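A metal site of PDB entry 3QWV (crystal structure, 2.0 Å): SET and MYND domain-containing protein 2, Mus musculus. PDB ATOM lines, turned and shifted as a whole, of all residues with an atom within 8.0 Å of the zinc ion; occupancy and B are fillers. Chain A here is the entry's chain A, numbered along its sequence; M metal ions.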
ATOM      1  N   HIS A  51       5.959 -13.914   5.359  1.00  0.00           N
ATOM      2  CA  HIS A  51       4.566 -13.845   5.792  1.00  0.00           C
ATOM      3  C   HIS A  51       4.386 -12.717   6.798  1.00  0.00           C
ATOM      4  O   HIS A  51       5.307 -12.402   7.583  1.00  0.00           O
ATOM      5  CB  HIS A  51       4.149 -15.157   6.459  1.00  0.00           C
ATOM      6  CG  HIS A  51       3.953 -16.280   5.498  1.00  0.00           C
ATOM      7  ND1 HIS A  51       5.021 -16.999   5.009  1.00  0.00           N
ATOM      8  CD2 HIS A  51       2.806 -16.825   5.027  1.00  0.00           C
ATOM      9  CE1 HIS A  51       4.497 -17.909   4.194  1.00  0.00           C
ATOM     10  NE2 HIS A  51       3.165 -17.844   4.184  1.00  0.00           N
ATOM     11  N   CYS A  52       3.229 -12.082   6.762  1.00  0.00           N
ATOM     12  CA  CYS A  52       2.912 -10.984   7.682  1.00  0.00           C
ATOM     13  C   CYS A  52       2.852 -11.544   9.106  1.00  0.00           C
ATOM     14  O   CYS A  52       2.158 -12.526   9.331  1.00  0.00           O
ATOM     15  CB  CYS A  52       1.593 -10.327   7.287  1.00  0.00           C
ATOM     16  SG  CYS A  52       0.993  -9.103   8.473  1.00  0.00           S
ATOM     17  N   GLU A  53       3.567 -10.914  10.035  1.00  0.00           N
ATOM     18  CA  GLU A  53       3.664 -11.291  11.450  1.00  0.00           C
ATOM     19  C   GLU A  53       2.264 -11.259  12.089  1.00  0.00           C
ATOM     20  O   GLU A  53       1.991 -11.986  13.040  1.00  0.00           O
ATOM     21  CB  GLU A  53       4.626 -10.285  12.165  1.00  0.00           C
ATOM     22  CG  GLU A  53       5.639 -10.896  13.113  1.00  0.00           C
ATOM     23  CD  GLU A  53       6.956 -11.420  12.569  1.00  0.00           C
ATOM     24  OE1 GLU A  53       7.448 -10.916  11.525  1.00  0.00           O
ATOM     25  OE2 GLU A  53       7.534 -12.289  13.251  1.00  0.00           O
ATOM     26  N   CYS A  54       1.381 -10.418  11.575  1.00  0.00           N
ATOM     27  CA  CYS A  54       0.050 -10.307  12.151  1.00  0.00           C
ATOM     28  C   CYS A  54      -0.945 -11.340  11.594  1.00  0.00           C
ATOM     29  O   CYS A  54      -1.419 -12.183  12.350  1.00  0.00           O
ATOM     30  CB  CYS A  54      -0.470  -8.870  12.005  1.00  0.00           C
ATOM     31  SG  CYS A  54      -2.134  -8.608  12.633  1.00  0.00           S
ATOM     32  N   CYS A  55      -1.275 -11.268  10.297  1.00  0.00           N
ATOM     33  CA  CYS A  55      -2.311 -12.068   9.638  1.00  0.00           C
ATOM     34  C   CYS A  55      -1.798 -13.311   8.887  1.00  0.00           C
ATOM     35  O   CYS A  55      -2.600 -14.006   8.274  1.00  0.00           O
ATOM     36  CB  CYS A  55      -3.117 -11.172   8.716  1.00  0.00           C
ATOM     37  SG  CYS A  55      -2.270 -10.817   7.157  1.00  0.00           S
ATOM     38  N   PHE A  56      -0.487 -13.527   8.862  1.00  0.00           N
ATOM     39  CA  PHE A  56       0.134 -14.660   8.190  1.00  0.00           C
ATOM     40  C   PHE A  56       0.032 -14.631   6.637  1.00  0.00           C
ATOM     41  O   PHE A  56       0.308 -15.653   6.019  1.00  0.00           O
ATOM     42  CB  PHE A  56      -0.370 -16.014   8.765  1.00  0.00           C
ATOM     43  CG  PHE A  56       0.150 -16.448  10.130  1.00  0.00           C
ATOM     44  CD1 PHE A  56       0.449 -15.503  11.115  1.00  0.00           C
ATOM     45  CD2 PHE A  56       0.270 -17.799  10.452  1.00  0.00           C
ATOM     46  CE1 PHE A  56       0.851 -15.913  12.407  1.00  0.00           C
ATOM     47  CE2 PHE A  56       0.716 -18.204  11.717  1.00  0.00           C
ATOM     48  CZ  PHE A  56       0.980 -17.262  12.694  1.00  0.00           C
ATOM     49  N   ALA A  57      -0.383 -13.512   6.016  1.00  0.00           N
ATOM     50  CA  ALA A  57      -0.475 -13.434   4.546  1.00  0.00           C
ATOM     51  C   ALA A  57       0.891 -13.602   3.895  1.00  0.00           C
ATOM     52  O   ALA A  57       1.882 -13.057   4.377  1.00  0.00           O
ATOM     53  CB  ALA A  57      -1.095 -12.136   4.098  1.00  0.00           C
ATOM     54  N   ARG A  58       0.941 -14.399   2.819  1.00  0.00           N
ATOM     55  CA  ARG A  58       2.163 -14.631   2.070  1.00  0.00           C
ATOM     56  C   ARG A  58       2.236 -13.519   1.017  1.00  0.00           C
ATOM     57  O   ARG A  58       1.396 -13.458   0.120  1.00  0.00           O
ATOM     58  CB  ARG A  58       2.166 -16.025   1.403  1.00  0.00           C
ATOM     59  CG  ARG A  58       3.502 -16.366   0.757  1.00  0.00           C
ATOM     60  CD  ARG A  58       3.507 -17.694   0.021  1.00  0.00           C
ATOM     61  NE  ARG A  58       2.451 -17.781  -0.985  1.00  0.00           N
ATOM     62  CZ  ARG A  58       2.601 -17.519  -2.277  1.00  0.00           C
ATOM     63  NH1 ARG A  58       3.787 -17.148  -2.746  1.00  0.00           N
ATOM     64  NH2 ARG A  58       1.579 -17.631  -3.115  1.00  0.00           N
ATOM     65  N   LYS A  59       3.217 -12.629   1.156  1.00  0.00           N
ATOM     66  CA  LYS A  59       3.377 -11.455   0.286  1.00  0.00           C
ATOM     67  C   LYS A  59       4.817 -11.072   0.093  1.00  0.00           C
ATOM     68  O   LYS A  59       5.665 -11.289   0.980  1.00  0.00           O
ATOM     69  CB  LYS A  59       2.650 -10.238   0.880  1.00  0.00           C
ATOM     70  CG  LYS A  59       1.187 -10.131   0.507  1.00  0.00           C
ATOM     71  CD  LYS A  59       0.500  -8.968   1.228  1.00  0.00           C
ATOM     72  CE  LYS A  59      -1.004  -9.053   1.052  1.00  0.00           C
ATOM     73  NZ  LYS A  59      -1.701  -7.900   1.682  1.00  0.00           N
ATOM     74  N   LEU A  62       6.657  -6.836   2.014  1.00  0.00           N
ATOM     75  CA  LEU A  62       6.099  -6.602   3.351  1.00  0.00           C
ATOM     76  C   LEU A  62       6.878  -5.426   3.964  1.00  0.00           C
ATOM     77  O   LEU A  62       8.079  -5.286   3.703  1.00  0.00           O
ATOM     78  CB  LEU A  62       6.281  -7.838   4.244  1.00  0.00           C
ATOM     79  CG  LEU A  62       5.414  -9.056   3.910  1.00  0.00           C
ATOM     80  CD1 LEU A  62       5.886 -10.265   4.683  1.00  0.00           C
ATOM     81  CD2 LEU A  62       3.912  -8.757   4.136  1.00  0.00           C
ATOM     82  N   PHE A  72       7.693  -7.999  10.054  1.00  0.00           N
ATOM     83  CA  PHE A  72       7.227  -7.577   8.728  1.00  0.00           C
ATOM     84  C   PHE A  72       5.732  -7.733   8.651  1.00  0.00           C
ATOM     85  O   PHE A  72       5.170  -8.700   9.173  1.00  0.00           O
ATOM     86  CB  PHE A  72       7.916  -8.401   7.638  1.00  0.00           C
ATOM     87  CG  PHE A  72       9.416  -8.282   7.547  1.00  0.00           C
ATOM     88  CD1 PHE A  72      10.246  -8.969   8.436  1.00  0.00           C
ATOM     89  CD2 PHE A  72      10.017  -7.535   6.529  1.00  0.00           C
ATOM     90  CE1 PHE A  72      11.632  -8.886   8.328  1.00  0.00           C
ATOM     91  CE2 PHE A  72      11.413  -7.461   6.421  1.00  0.00           C
ATOM     92  CZ  PHE A  72      12.214  -8.138   7.317  1.00  0.00           C
ATOM     93  N   TYR A  73       5.068  -6.748   8.039  1.00  0.00           N
ATOM     94  CA  TYR A  73       3.623  -6.596   7.963  1.00  0.00           C
ATOM     95  C   TYR A  73       3.107  -6.254   6.596  1.00  0.00           C
ATOM     96  O   TYR A  73       3.832  -5.685   5.791  1.00  0.00           O
ATOM     97  CB  TYR A  73       3.206  -5.480   8.925  1.00  0.00           C
ATOM     98  CG  TYR A  73       3.580  -5.766  10.362  1.00  0.00           C
ATOM     99  CD1 TYR A  73       2.882  -6.708  11.100  1.00  0.00           C
ATOM    100  CD2 TYR A  73       4.651  -5.111  10.965  1.00  0.00           C
ATOM    101  CE1 TYR A  73       3.211  -6.968  12.428  1.00  0.00           C
ATOM    102  CE2 TYR A  73       4.993  -5.369  12.300  1.00  0.00           C
ATOM    103  CZ  TYR A  73       4.279  -6.305  13.020  1.00  0.00           C
ATOM    104  OH  TYR A  73       4.557  -6.590  14.328  1.00  0.00           O
ATOM    105  N   CYS A  74       1.809  -6.528   6.346  1.00  0.00           N
ATOM    106  CA  CYS A  74       1.145  -6.178   5.073  1.00  0.00           C
ATOM    107  C   CYS A  74       1.250  -4.695   4.826  1.00  0.00           C
ATOM    108  O   CYS A  74       1.502  -4.251   3.707  1.00  0.00           O
ATOM    109  CB  CYS A  74      -0.328  -6.585   5.109  1.00  0.00           C
ATOM    110  SG  CYS A  74      -0.616  -8.360   5.150  1.00  0.00           S
ATOM    111  N   ASP A  75       0.963  -3.923   5.894  1.00  0.00           N
ATOM    112  CA  ASP A  75       0.856  -2.476   5.871  1.00  0.00           C
ATOM    113  C   ASP A  75       0.833  -1.994   7.332  1.00  0.00           C
ATOM    114  O   ASP A  75       0.933  -2.816   8.249  1.00  0.00           O
ATOM    115  CB  ASP A  75      -0.475  -2.085   5.149  1.00  0.00           C
ATOM    116  CG  ASP A  75      -1.731  -2.854   5.580  1.00  0.00           C
ATOM    117  OD1 ASP A  75      -1.792  -3.313   6.765  1.00  0.00           O
ATOM    118  OD2 ASP A  75      -2.712  -2.904   4.789  1.00  0.00           O
ATOM    119  N   GLU A  77      -1.703  -1.046   9.037  1.00  0.00           N
ATOM    120  CA  GLU A  77      -2.888  -1.548   9.751  1.00  0.00           C
ATOM    121  C   GLU A  77      -2.584  -2.865  10.456  1.00  0.00           C
ATOM    122  O   GLU A  77      -2.957  -3.012  11.628  1.00  0.00           O
ATOM    123  CB  GLU A  77      -4.085  -1.675   8.805  1.00  0.00           C
ATOM    124  CG  GLU A  77      -4.614  -0.320   8.333  1.00  0.00           C
ATOM    125  CD  GLU A  77      -3.980   0.287   7.097  1.00  0.00           C
ATOM    126  OE1 GLU A  77      -2.871  -0.144   6.703  1.00  0.00           O
ATOM    127  OE2 GLU A  77      -4.608   1.197   6.510  1.00  0.00           O
ATOM    128  N   CYS A  78      -1.845  -3.792   9.783  1.00  0.00           N
ATOM    129  CA  CYS A  78      -1.444  -5.067  10.390  1.00  0.00           C
ATOM    130  C   CYS A  78      -0.355  -4.772  11.457  1.00  0.00           C
ATOM    131  O   CYS A  78      -0.343  -5.391  12.511  1.00  0.00           O
ATOM    132  CB  CYS A  78      -0.984  -6.078   9.346  1.00  0.00           C
ATOM    133  SG  CYS A  78      -2.302  -7.160   8.720  1.00  0.00           S
ATOM    134  N   GLN A  79       0.510  -3.765  11.198  1.00  0.00           N
ATOM    135  CA  GLN A  79       1.543  -3.324  12.134  1.00  0.00           C
ATOM    136  C   GLN A  79       0.916  -2.793  13.429  1.00  0.00           C
ATOM    137  O   GLN A  79       1.406  -3.137  14.502  1.00  0.00           O
ATOM    138  CB  GLN A  79       2.462  -2.285  11.502  1.00  0.00           C
ATOM    139  CG  GLN A  79       3.634  -1.878  12.417  1.00  0.00           C
ATOM    140  CD  GLN A  79       4.551  -0.861  11.781  1.00  0.00           C
ATOM    141  OE1 GLN A  79       5.659  -0.603  12.253  1.00  0.00           O
ATOM    142  NE2 GLN A  79       4.121  -0.265  10.684  1.00  0.00           N
ATOM    143  N   GLU A  81      -2.249  -3.477  14.580  1.00  0.00           N
ATOM    144  CA  GLU A  81      -2.963  -4.576  15.206  1.00  0.00           C
ATOM    145  C   GLU A  81      -1.987  -5.451  16.031  1.00  0.00           C
ATOM    146  O   GLU A  81      -2.309  -5.815  17.146  1.00  0.00           O
ATOM    147  CB  GLU A  81      -3.665  -5.451  14.142  1.00  0.00           C
ATOM    148  CG  GLU A  81      -4.553  -6.519  14.780  1.00  0.00           C
ATOM    149  CD  GLU A  81      -5.239  -7.531  13.881  1.00  0.00           C
ATOM    150  OE1 GLU A  81      -5.497  -7.240  12.694  1.00  0.00           O
ATOM    151  OE2 GLU A  81      -5.565  -8.628  14.403  1.00  0.00           O
HETATM  152 ZN    ZN M   1      -1.109  -8.712   7.505  1.00  0.00          ZN
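Of the 18 residues printed, 4 come within 4 Å of the zinc ion.
The nearest printed residue that does not touch the zinc ion is Cys 54 (4.5 Å).
The side-chain sulfur (SG) of Cys 54 sits close to the backbone carbonyl oxygen (O) of Cys 78 (3.7 Å).
SG of Cys 55 sits close to N of Ala 57.
NZ of Lys 59 lies close to SG of Cys 74, 3.7 Å away.
N of Cys 78 lies within hydrogen-bond range of OD1 of Asp 75 (3.1 Å).
The side-chain sulfur (SG) of Cys 52 lies close to the backbone NH (N) of Cys 54 (3.4 Å).
The backbone NH (N) of Cys 52 sits at hydrogen-bond distance from the backbone carbonyl oxygen (O) of Ala 57 (2.9 Å).
SG of Cys 78 is bound to the zinc ion, 2.3 Å away.
The zinc ion is bound by SG of Cys 52 (2.3 Å).
The zinc ion is bound by SG of Cys 55, 2.4 Å away.
SG of Cys 74 binds the zinc ion.
The zinc ion has four donor atoms within binding distance.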
